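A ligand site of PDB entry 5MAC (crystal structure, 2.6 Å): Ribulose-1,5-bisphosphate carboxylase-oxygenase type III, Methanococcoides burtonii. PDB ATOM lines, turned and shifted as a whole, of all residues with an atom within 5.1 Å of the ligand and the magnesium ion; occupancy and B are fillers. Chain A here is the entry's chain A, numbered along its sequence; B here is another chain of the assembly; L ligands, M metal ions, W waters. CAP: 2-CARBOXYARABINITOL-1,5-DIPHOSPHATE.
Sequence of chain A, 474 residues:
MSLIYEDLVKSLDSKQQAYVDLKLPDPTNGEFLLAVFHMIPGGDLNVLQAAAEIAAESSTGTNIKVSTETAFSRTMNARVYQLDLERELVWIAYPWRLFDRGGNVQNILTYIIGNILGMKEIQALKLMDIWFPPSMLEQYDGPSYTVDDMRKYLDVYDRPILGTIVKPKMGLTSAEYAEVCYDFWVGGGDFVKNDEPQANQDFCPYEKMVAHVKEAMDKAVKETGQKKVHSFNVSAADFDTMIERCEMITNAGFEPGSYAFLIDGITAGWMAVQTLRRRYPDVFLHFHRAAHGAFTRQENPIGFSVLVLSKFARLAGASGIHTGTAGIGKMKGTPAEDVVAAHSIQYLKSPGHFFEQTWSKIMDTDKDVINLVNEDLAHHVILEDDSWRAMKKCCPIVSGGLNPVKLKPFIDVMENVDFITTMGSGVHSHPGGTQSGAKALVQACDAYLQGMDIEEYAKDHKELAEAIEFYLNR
The magnesium ion is bound by an oxygen (O7) of the ligand (1.9 Å), an oxygen (O2) of the ligand (2.0 Å), the side-chain carboxylate of Glu 196 (2.1 Å), an oxygen (O3) of the ligand (2.2 Å), the side-chain carboxylate of Asp 195 (2.2 Å) and OQ2 of KCX 193 (2.2 Å). The magnesium ion has six donor atoms within binding distance.
Residues that only touch the magnesium ion: Lys 167 (3.97 Å) and Asn 115 of chain B (3.4 Å). Within 4 Å of the magnesium ion: Lys 167, KCX 193, Asp 195, Glu 196 and Asn 115 of chain B.
Water W2 lies within hydrogen-bond range of O6P of the ligand (2.6 Å), N of Arg 289 (2.9 Å), NE2 of His 288 (3.0 Å) and ND1 of His 322 (3.3 Å). Water W8 lies within hydrogen-bond range of the backbone carbonyl oxygen (O) of Ile 397 (2.6 Å), an oxygen (O4P) of the ligand (2.7 Å), the backbone NH (N) of Gly 324 (2.9 Å), the backbone NH (N) of Ser 399 (3.0 Å) and a ring nitrogen (ND1) of His 322 (3.4 Å). Water W1 lies within hydrogen-bond range of the backbone carbonyl oxygen (O) of Leu 402 (2.6 Å), an oxygen (O1P) of the ligand (2.7 Å), the backbone NH (N) of Gly 426 (2.7 Å), the side-chain hydroxyl (OG) of Ser 425 (3.1 Å) and the backbone NH (N) of Gly 424 (3.4 Å). Water W6 lies within hydrogen-bond range of NE2 of His 292 (2.7 Å) and O5P of the ligand (2.8 Å). Water W4 bridges the backbone carbonyl oxygen (O) of Ser 399 (2.7 Å) and an oxygen (O5P) of the ligand (2.8 Å). Water W7 lies within hydrogen-bond range of OD1 of Asn 115 of chain B, O6P of the ligand and NE2 of His 292.
Merely in contact with the ligand: Ile 165, Glu 57 of chain B, Met 331 and Met 423. Within 4 Å of the ligand: Ile 165, Lys 167, Lys 169, KCX 193, Asp 195, Glu 196, His 288, Arg 289, His 322, Lys 330, Met 331, Ser 399, Gly 400, Gly 401, Met 423, Gly 424, Ser 425, Glu 57 of chain B, Thr 62 of chain B and Asn 115 of chain B. The nearest printed residue that does not touch the ligand is Thr 422 (4.1 Å).
The side-chain carboxylate of Glu 196 sits close to a ring nitrogen (NE2) of His 288, at 3.4 Å. The side-chain amino group (NZ) of Lys 169 lies within salt-bridge range of the side-chain carboxylate (OE2) of Glu 196. OD2 of Asp 195 lies within salt-bridge range of NZ of Lys 167 (2.7 Å). The side-chain amino group of Lys 330 lies within salt-bridge range of the side-chain carboxylate of Glu 57 of chain B, 2.8 Å away. O of His 322 lies close to NE of Arg 289 (3.5 Å). The side-chain hydroxyl (OG) of Ser 399 lies within hydrogen-bond range of the side-chain hydroxyl (OG1) of Thr 422 (3.1 Å). The side-chain amino group (NZ) of Lys 169 lies within salt-bridge range of the side-chain carboxylate (OE1) of Glu 57 of chain B (3.9 Å). The side-chain carboxylate (OE2) of Glu 57 of chain B lies within hydrogen-bond range of the backbone NH (N) of Asn 63 of chain B (3.3 Å).
NE2 of His 288 lies close to O3 of the ligand (2.6 Å). O2P of the ligand lies within hydrogen-bond range of OG1 of Thr 62 of chain B (2.7 Å). NZ of Lys 330 is in salt-bridge range of O3P of the ligand (2.7 Å). N of Gly 401 sits at hydrogen-bond distance from O3P of the ligand (2.8 Å). The backbone NH (N) of Gly 400 is in hydrogen-bond range of an oxygen (O4) of the ligand, 2.9 Å away. The backbone NH (N) of Gly 424 is in hydrogen-bond range of an oxygen (O1P) of the ligand, 2.9 Å away. A ring nitrogen (ND1) of His 322 lies within hydrogen-bond range of an oxygen (O4P) of the ligand (2.9 Å). NH2 of Arg 289 is in salt-bridge range of O5P of the ligand (2.9 Å). N of Ser 425 lies within hydrogen-bond range of O2P of the ligand (2.9 Å). ND2 of Asn 115 of chain B lies close to O3 of the ligand (3.1 Å). The backbone carbonyl oxygen (O) of Ser 399 sits close to an oxygen (O4) of the ligand, 3.4 Å away. The side-chain hydroxyl (OG) of Ser 399 sits close to an oxygen (O4) of the ligand. O2P of the ligand lies within salt-bridge range of NZ of Lys 167 (3.6 Å). O7 of the ligand sits close to NZ of Lys 169 (3.3 Å).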
ATOM      1  N   ILE A 165     -22.243  24.143  -3.423  1.00  0.00           N
ATOM      2  CA  ILE A 165     -22.937  25.160  -2.648  1.00  0.00           C
ATOM      3  C   ILE A 165     -22.875  24.608  -1.240  1.00  0.00           C
ATOM      4  O   ILE A 165     -23.030  23.405  -1.047  1.00  0.00           O
ATOM      5  CB  ILE A 165     -24.412  25.342  -3.074  1.00  0.00           C
ATOM      6  CG1 ILE A 165     -24.605  25.415  -4.588  1.00  0.00           C
ATOM      7  CG2 ILE A 165     -24.989  26.563  -2.381  1.00  0.00           C
ATOM      8  CD1 ILE A 165     -25.086  24.113  -5.203  1.00  0.00           C
ATOM      9  N   LYS A 167     -24.275  23.593   2.175  1.00  0.00           N
ATOM     10  CA  LYS A 167     -25.555  23.131   2.706  1.00  0.00           C
ATOM     11  C   LYS A 167     -25.378  22.656   4.159  1.00  0.00           C
ATOM     12  O   LYS A 167     -24.332  22.094   4.465  1.00  0.00           O
ATOM     13  CB  LYS A 167     -26.084  21.969   1.857  1.00  0.00           C
ATOM     14  CG  LYS A 167     -26.283  22.297   0.393  1.00  0.00           C
ATOM     15  CD  LYS A 167     -27.403  23.290   0.114  1.00  0.00           C
ATOM     16  CE  LYS A 167     -27.497  23.626  -1.351  1.00  0.00           C
ATOM     17  NZ  LYS A 167     -28.744  24.335  -1.704  1.00  0.00           N
ATOM     18  N   LYS A 169     -28.803  25.145   3.666  1.00  0.00           N
ATOM     19  CA  LYS A 169     -29.050  26.458   3.055  1.00  0.00           C
ATOM     20  C   LYS A 169     -28.971  27.589   4.100  1.00  0.00           C
ATOM     21  O   LYS A 169     -28.587  28.717   3.778  1.00  0.00           O
ATOM     22  CB  LYS A 169     -30.403  26.459   2.343  1.00  0.00           C
ATOM     23  CG  LYS A 169     -30.842  27.806   1.770  1.00  0.00           C
ATOM     24  CD  LYS A 169     -32.150  27.675   1.020  1.00  0.00           C
ATOM     25  CE  LYS A 169     -32.022  26.803  -0.169  1.00  0.00           C
ATOM     26  NZ  LYS A 169     -32.764  27.322  -1.337  1.00  0.00           N
ATOM     27  N   KCX A 193     -19.594  28.084  -3.578  1.00  0.00           N
ATOM     28  CA  KCX A 193     -20.483  29.243  -3.636  1.00  0.00           C
ATOM     29  CB  KCX A 193     -21.378  29.371  -4.902  1.00  0.00           C
ATOM     30  CG  KCX A 193     -22.461  28.305  -5.016  1.00  0.00           C
ATOM     31  CD  KCX A 193     -23.338  28.536  -6.248  1.00  0.00           C
ATOM     32  CE  KCX A 193     -24.253  29.753  -5.974  1.00  0.00           C
ATOM     33  NZ  KCX A 193     -25.331  29.533  -4.952  1.00  0.00           N
ATOM     34  C   KCX A 193     -21.356  29.318  -2.386  1.00  0.00           C
ATOM     35  O   KCX A 193     -21.723  28.285  -1.798  1.00  0.00           O
ATOM     36  CX  KCX A 193     -26.447  28.752  -5.167  1.00  0.00           C
ATOM     37  OQ1 KCX A 193     -26.653  28.183  -6.206  1.00  0.00           O
ATOM     38  OQ2 KCX A 193     -27.337  28.583  -4.216  1.00  0.00           O
ATOM     39  N   ASP A 195     -24.795  29.575  -0.681  1.00  0.00           N
ATOM     40  CA  ASP A 195     -26.207  29.375  -1.075  1.00  0.00           C
ATOM     41  C   ASP A 195     -26.853  30.788  -1.088  1.00  0.00           C
ATOM     42  O   ASP A 195     -26.565  31.602  -0.209  1.00  0.00           O
ATOM     43  CB  ASP A 195     -26.950  28.427  -0.112  1.00  0.00           C
ATOM     44  CG  ASP A 195     -27.981  27.546  -0.754  1.00  0.00           C
ATOM     45  OD1 ASP A 195     -28.480  27.902  -1.838  1.00  0.00           O
ATOM     46  OD2 ASP A 195     -28.293  26.501  -0.191  1.00  0.00           O
ATOM     47  N   GLU A 196     -27.653  31.104  -2.121  1.00  0.00           N
ATOM     48  CA  GLU A 196     -28.215  32.451  -2.360  1.00  0.00           C
ATOM     49  C   GLU A 196     -28.702  33.261  -1.133  1.00  0.00           C
ATOM     50  O   GLU A 196     -28.585  34.482  -1.222  1.00  0.00           O
ATOM     51  CB  GLU A 196     -29.343  32.438  -3.405  1.00  0.00           C
ATOM     52  CG  GLU A 196     -30.626  31.739  -3.024  1.00  0.00           C
ATOM     53  CD  GLU A 196     -30.581  30.226  -2.957  1.00  0.00           C
ATOM     54  OE1 GLU A 196     -29.671  29.626  -3.572  1.00  0.00           O
ATOM     55  OE2 GLU A 196     -31.454  29.643  -2.290  1.00  0.00           O
ATOM     56  N   HIS A 288     -27.036  35.005  -9.488  1.00  0.00           N
ATOM     57  CA  HIS A 288     -27.973  34.020  -9.017  1.00  0.00           C
ATOM     58  C   HIS A 288     -29.365  34.610  -9.430  1.00  0.00           C
ATOM     59  O   HIS A 288     -29.545  35.837  -9.370  1.00  0.00           O
ATOM     60  CB  HIS A 288     -27.871  33.764  -7.496  1.00  0.00           C
ATOM     61  CG  HIS A 288     -28.524  32.480  -7.129  1.00  0.00           C
ATOM     62  ND1 HIS A 288     -29.874  32.407  -6.862  1.00  0.00           N
ATOM     63  CD2 HIS A 288     -28.011  31.220  -7.120  1.00  0.00           C
ATOM     64  CE1 HIS A 288     -30.127  31.124  -6.656  1.00  0.00           C
ATOM     65  NE2 HIS A 288     -29.046  30.379  -6.828  1.00  0.00           N
ATOM     66  N   ARG A 289     -30.298  33.746  -9.911  1.00  0.00           N
ATOM     67  CA  ARG A 289     -31.588  34.159 -10.487  1.00  0.00           C
ATOM     68  C   ARG A 289     -32.830  33.747  -9.661  1.00  0.00           C
ATOM     69  O   ARG A 289     -33.939  33.726 -10.194  1.00  0.00           O
ATOM     70  CB  ARG A 289     -31.703  33.641 -11.970  1.00  0.00           C
ATOM     71  CG  ARG A 289     -31.575  32.125 -12.123  1.00  0.00           C
ATOM     72  CD  ARG A 289     -31.872  31.678 -13.541  1.00  0.00           C
ATOM     73  NE  ARG A 289     -32.024  30.217 -13.608  1.00  0.00           N
ATOM     74  CZ  ARG A 289     -32.463  29.548 -14.660  1.00  0.00           C
ATOM     75  NH1 ARG A 289     -32.764  30.193 -15.787  1.00  0.00           N
ATOM     76  NH2 ARG A 289     -32.593  28.235 -14.616  1.00  0.00           N
ATOM     77  N   HIS A 292     -36.930  34.111 -10.682  1.00  0.00           N
ATOM     78  CA  HIS A 292     -37.113  34.231 -12.138  1.00  0.00           C
ATOM     79  C   HIS A 292     -38.328  33.441 -12.675  1.00  0.00           C
ATOM     80  O   HIS A 292     -38.881  33.809 -13.724  1.00  0.00           O
ATOM     81  CB  HIS A 292     -35.822  33.806 -12.879  1.00  0.00           C
ATOM     82  CG  HIS A 292     -35.573  32.328 -12.885  1.00  0.00           C
ATOM     83  ND1 HIS A 292     -35.979  31.542 -13.944  1.00  0.00           N
ATOM     84  CD2 HIS A 292     -35.008  31.525 -11.957  1.00  0.00           C
ATOM     85  CE1 HIS A 292     -35.659  30.297 -13.605  1.00  0.00           C
ATOM     86  NE2 HIS A 292     -35.074  30.253 -12.424  1.00  0.00           N
ATOM     87  N   HIS A 322     -26.945  31.615 -13.944  1.00  0.00           N
ATOM     88  CA  HIS A 322     -27.558  30.301 -13.892  1.00  0.00           C
ATOM     89  C   HIS A 322     -28.488  30.170 -15.092  1.00  0.00           C
ATOM     90  O   HIS A 322     -29.205  31.103 -15.427  1.00  0.00           O
ATOM     91  CB  HIS A 322     -28.316  30.089 -12.590  1.00  0.00           C
ATOM     92  CG  HIS A 322     -27.455  29.893 -11.378  1.00  0.00           C
ATOM     93  ND1 HIS A 322     -27.493  28.708 -10.675  1.00  0.00           N
ATOM     94  CD2 HIS A 322     -26.579  30.714 -10.789  1.00  0.00           C
ATOM     95  CE1 HIS A 322     -26.622  28.846  -9.681  1.00  0.00           C
ATOM     96  NE2 HIS A 322     -26.046  30.039  -9.713  1.00  0.00           N
ATOM     97  N   GLY A 324     -29.806  26.632 -15.871  1.00  0.00           N
ATOM     98  CA  GLY A 324     -30.556  25.417 -15.650  1.00  0.00           C
ATOM     99  C   GLY A 324     -29.920  24.145 -16.186  1.00  0.00           C
ATOM    100  O   GLY A 324     -29.033  24.186 -17.029  1.00  0.00           O
ATOM    101  N   LYS A 330     -33.770  19.189 -10.452  1.00  0.00           N
ATOM    102  CA  LYS A 330     -35.029  19.540  -9.770  1.00  0.00           C
ATOM    103  C   LYS A 330     -35.788  20.787 -10.277  1.00  0.00           C
ATOM    104  O   LYS A 330     -36.887  21.058  -9.769  1.00  0.00           O
ATOM    105  CB  LYS A 330     -34.756  19.712  -8.256  1.00  0.00           C
ATOM    106  CG  LYS A 330     -34.235  21.081  -7.809  1.00  0.00           C
ATOM    107  CD  LYS A 330     -33.707  20.996  -6.419  1.00  0.00           C
ATOM    108  CE  LYS A 330     -33.075  22.280  -5.948  1.00  0.00           C
ATOM    109  NZ  LYS A 330     -32.335  22.081  -4.684  1.00  0.00           N
ATOM    110  N   MET A 331     -35.233  21.546 -11.253  1.00  0.00           N
ATOM    111  CA  MET A 331     -35.912  22.748 -11.776  1.00  0.00           C
ATOM    112  C   MET A 331     -36.438  22.513 -13.172  1.00  0.00           C
ATOM    113  O   MET A 331     -35.991  21.606 -13.867  1.00  0.00           O
ATOM    114  CB  MET A 331     -34.977  23.972 -11.765  1.00  0.00           C
ATOM    115  CG  MET A 331     -34.330  24.263 -10.434  1.00  0.00           C
ATOM    116  SD  MET A 331     -35.475  24.834  -9.161  1.00  0.00           S
ATOM    117  CE  MET A 331     -34.397  25.044  -7.819  1.00  0.00           C
ATOM    118  N   ILE A 397     -23.981  28.803 -15.412  1.00  0.00           N
ATOM    119  CA  ILE A 397     -23.770  28.136 -14.114  1.00  0.00           C
ATOM    120  C   ILE A 397     -24.885  27.070 -14.054  1.00  0.00           C
ATOM    121  O   ILE A 397     -26.041  27.398 -14.217  1.00  0.00           O
ATOM    122  CB  ILE A 397     -23.779  29.118 -12.932  1.00  0.00           C
ATOM    123  CG1 ILE A 397     -22.705  30.232 -13.191  1.00  0.00           C
ATOM    124  CG2 ILE A 397     -23.463  28.373 -11.630  1.00  0.00           C
ATOM    125  CD1 ILE A 397     -22.709  31.394 -12.300  1.00  0.00           C
ATOM    126  N   SER A 399     -26.814  24.394 -12.088  1.00  0.00           N
ATOM    127  CA  SER A 399     -27.120  24.002 -10.731  1.00  0.00           C
ATOM    128  C   SER A 399     -28.561  23.550 -10.628  1.00  0.00           C
ATOM    129  O   SER A 399     -29.334  23.835 -11.531  1.00  0.00           O
ATOM    130  CB  SER A 399     -26.888  25.223  -9.836  1.00  0.00           C
ATOM    131  OG  SER A 399     -26.800  24.905  -8.461  1.00  0.00           O
ATOM    132  N   GLY A 400     -28.909  22.882  -9.516  1.00  0.00           N
ATOM    133  CA  GLY A 400     -30.269  22.420  -9.209  1.00  0.00           C
ATOM    134  C   GLY A 400     -30.552  20.920  -9.231  1.00  0.00           C
ATOM    135  O   GLY A 400     -31.117  20.418 -10.178  1.00  0.00           O
ATOM    136  N   GLY A 401     -30.241  20.236  -8.153  1.00  0.00           N
ATOM    137  CA  GLY A 401     -30.567  18.828  -7.974  1.00  0.00           C
ATOM    138  C   GLY A 401     -29.765  17.853  -8.792  1.00  0.00           C
ATOM    139  O   GLY A 401     -30.263  16.772  -9.114  1.00  0.00           O
ATOM    140  N   LEU A 402     -28.500  18.183  -9.053  1.00  0.00           N
ATOM    141  CA  LEU A 402     -27.591  17.313  -9.816  1.00  0.00           C
ATOM    142  C   LEU A 402     -26.746  16.510  -8.876  1.00  0.00           C
ATOM    143  O   LEU A 402     -26.436  16.991  -7.792  1.00  0.00           O
ATOM    144  CB  LEU A 402     -26.638  18.150 -10.634  1.00  0.00           C
ATOM    145  CG  LEU A 402     -27.240  19.045 -11.683  1.00  0.00           C
ATOM    146  CD1 LEU A 402     -26.276  20.169 -12.022  1.00  0.00           C
ATOM    147  CD2 LEU A 402     -27.649  18.246 -12.902  1.00  0.00           C
ATOM    148  N   THR A 422     -22.470  23.383 -10.064  1.00  0.00           N
ATOM    149  CA  THR A 422     -22.475  23.331  -8.613  1.00  0.00           C
ATOM    150  C   THR A 422     -23.453  22.277  -8.165  1.00  0.00           C
ATOM    151  O   THR A 422     -24.592  22.246  -8.624  1.00  0.00           O
ATOM    152  CB  THR A 422     -22.689  24.711  -7.983  1.00  0.00           C
ATOM    153  OG1 THR A 422     -23.759  25.378  -8.613  1.00  0.00           O
ATOM    154  CG2 THR A 422     -21.446  25.559  -8.035  1.00  0.00           C
ATOM    155  N   MET A 423     -22.969  21.378  -7.315  1.00  0.00           N
ATOM    156  CA  MET A 423     -23.741  20.309  -6.716  1.00  0.00           C
ATOM    157  C   MET A 423     -23.666  20.416  -5.169  1.00  0.00           C
ATOM    158  O   MET A 423     -22.615  20.180  -4.588  1.00  0.00           O
ATOM    159  CB  MET A 423     -23.194  18.971  -7.220  1.00  0.00           C
ATOM    160  CG  MET A 423     -23.095  18.942  -8.677  1.00  0.00           C
ATOM    161  SD  MET A 423     -22.902  17.244  -9.240  1.00  0.00           S
ATOM    162  CE  MET A 423     -23.101  17.483 -10.992  1.00  0.00           C
ATOM    163  N   GLY A 424     -24.780  20.821  -4.545  1.00  0.00           N
ATOM    164  CA  GLY A 424     -24.885  20.924  -3.081  1.00  0.00           C
ATOM    165  C   GLY A 424     -25.334  19.592  -2.501  1.00  0.00           C
ATOM    166  O   GLY A 424     -24.531  18.887  -1.883  1.00  0.00           O
ATOM    167  N   SER A 425     -26.595  19.215  -2.731  1.00  0.00           N
ATOM    168  CA  SER A 425     -27.125  17.927  -2.246  1.00  0.00           C
ATOM    169  C   SER A 425     -26.387  16.746  -2.907  1.00  0.00           C
ATOM    170  O   SER A 425     -26.124  15.750  -2.242  1.00  0.00           O
ATOM    171  CB  SER A 425     -28.643  17.838  -2.454  1.00  0.00           C
ATOM    172  OG  SER A 425     -29.020  17.649  -3.806  1.00  0.00           O
ATOM    173  N   GLY A 426     -25.955  16.899  -4.154  1.00  0.00           N
ATOM    174  CA  GLY A 426     -25.202  15.863  -4.853  1.00  0.00           C
ATOM    175  C   GLY A 426     -23.782  15.649  -4.360  1.00  0.00           C
ATOM    176  O   GLY A 426     -23.067  14.835  -4.935  1.00  0.00           O
ATOM    177  N   GLU B  57     -36.738  23.878   0.606  1.00  0.00           N
ATOM    178  CA  GLU B  57     -36.049  24.752  -0.329  1.00  0.00           C
ATOM    179  C   GLU B  57     -36.176  26.248  -0.045  1.00  0.00           C
ATOM    180  O   GLU B  57     -35.373  27.009  -0.552  1.00  0.00           O
ATOM    181  CB  GLU B  57     -36.503  24.438  -1.738  1.00  0.00           C
ATOM    182  CG  GLU B  57     -36.146  23.029  -2.159  1.00  0.00           C
ATOM    183  CD  GLU B  57     -34.696  22.755  -2.430  1.00  0.00           C
ATOM    184  OE1 GLU B  57     -33.867  23.671  -2.304  1.00  0.00           O
ATOM    185  OE2 GLU B  57     -34.395  21.592  -2.808  1.00  0.00           O
ATOM    186  N   THR B  62     -32.551  20.954   1.326  1.00  0.00           N
ATOM    187  CA  THR B  62     -32.316  20.645  -0.071  1.00  0.00           C
ATOM    188  C   THR B  62     -32.929  19.305  -0.460  1.00  0.00           C
ATOM    189  O   THR B  62     -33.516  18.640   0.363  1.00  0.00           O
ATOM    190  CB  THR B  62     -30.839  20.766  -0.383  1.00  0.00           C
ATOM    191  OG1 THR B  62     -30.690  20.724  -1.835  1.00  0.00           O
ATOM    192  CG2 THR B  62     -30.008  19.720   0.379  1.00  0.00           C
ATOM    193  N   ASN B  63     -32.802  18.945  -1.744  1.00  0.00           N
ATOM    194  CA  ASN B  63     -33.410  17.776  -2.373  1.00  0.00           C
ATOM    195  C   ASN B  63     -33.191  16.411  -1.626  1.00  0.00           C
ATOM    196  O   ASN B  63     -34.070  15.541  -1.659  1.00  0.00           O
ATOM    197  CB  ASN B  63     -32.931  17.678  -3.844  1.00  0.00           C
ATOM    198  CG  ASN B  63     -33.794  16.806  -4.673  1.00  0.00           C
ATOM    199  OD1 ASN B  63     -33.386  15.715  -5.105  1.00  0.00           O
ATOM    200  ND2 ASN B  63     -35.032  17.273  -4.905  1.00  0.00           N
ATOM    201  N   ASN B 115     -36.164  30.440  -5.374  1.00  0.00           N
ATOM    202  CA  ASN B 115     -35.889  29.169  -6.055  1.00  0.00           C
ATOM    203  C   ASN B 115     -37.086  28.261  -6.176  1.00  0.00           C
ATOM    204  O   ASN B 115     -37.228  27.588  -7.186  1.00  0.00           O
ATOM    205  CB  ASN B 115     -34.737  28.416  -5.369  1.00  0.00           C
ATOM    206  CG  ASN B 115     -33.343  28.879  -5.750  1.00  0.00           C
ATOM    207  OD1 ASN B 115     -33.137  29.515  -6.796  1.00  0.00           O
ATOM    208  ND2 ASN B 115     -32.354  28.504  -4.954  1.00  0.00           N
HETATM  209  C1  CAP L   1     -28.790  24.203  -5.848  1.00  0.00           C
HETATM  210  C2  CAP L   1     -29.273  25.586  -5.392  1.00  0.00           C
HETATM  211  C3  CAP L   1     -29.395  26.599  -6.545  1.00  0.00           C
HETATM  212  C4  CAP L   1     -30.450  26.326  -7.625  1.00  0.00           C
HETATM  213  C5  CAP L   1     -30.779  27.573  -8.416  1.00  0.00           C
HETATM  214  C   CAP L   1     -30.557  25.532  -4.579  1.00  0.00           C
HETATM  215  O1  CAP L   1     -28.559  23.339  -4.743  1.00  0.00           O
HETATM  216  O2  CAP L   1     -28.237  26.043  -4.520  1.00  0.00           O
HETATM  217  O3  CAP L   1     -29.524  27.925  -6.011  1.00  0.00           O
HETATM  218  O4  CAP L   1     -29.972  25.354  -8.542  1.00  0.00           O
HETATM  219  O5  CAP L   1     -31.620  27.210  -9.513  1.00  0.00           O
HETATM  220  O6  CAP L   1     -31.512  24.780  -4.882  1.00  0.00           O
HETATM  221  O7  CAP L   1     -30.648  26.278  -3.579  1.00  0.00           O
HETATM  222  P1  CAP L   1     -28.613  21.732  -4.914  1.00  0.00           P
HETATM  223  P2  CAP L   1     -31.200  27.666 -10.984  1.00  0.00           P
HETATM  224  O1P CAP L   1     -27.348  21.394  -5.687  1.00  0.00           O
HETATM  225  O2P CAP L   1     -28.632  21.193  -3.508  1.00  0.00           O
HETATM  226  O3P CAP L   1     -29.885  21.401  -5.638  1.00  0.00           O
HETATM  227  O4P CAP L   1     -29.841  27.016 -11.138  1.00  0.00           O
HETATM  228  O5P CAP L   1     -32.221  27.086 -11.932  1.00  0.00           O
HETATM  229  O6P CAP L   1     -31.254  29.188 -10.910  1.00  0.00           O
HETATM  230 MG    MG M   1     -29.287  27.618  -3.867  1.00  0.00          MG
HETATM  231  O   HOH W   1     -27.028  18.699  -5.913  1.00  0.00           O
HETATM  232  O   HOH W   2     -29.750  30.950  -9.713  1.00  0.00           O
HETATM  233  O   HOH W   3     -26.946  21.009  -8.203  1.00  0.00           O
HETATM  234  O   HOH W   4     -31.816  24.346 -12.417  1.00  0.00           O
HETATM  235  O   HOH W   5     -33.787  26.141  -3.535  1.00  0.00           O
HETATM  236  O   HOH W   6     -34.950  27.631 -11.779  1.00  0.00           O
HETATM  237  O   HOH W   7     -33.552  29.984  -9.473  1.00  0.00           O
HETATM  238  O   HOH W   8     -28.337  26.692 -13.323  1.00  0.00           O
HETATM  239  O   HOH W   9     -31.338  23.852  -1.345  1.00  0.00           O
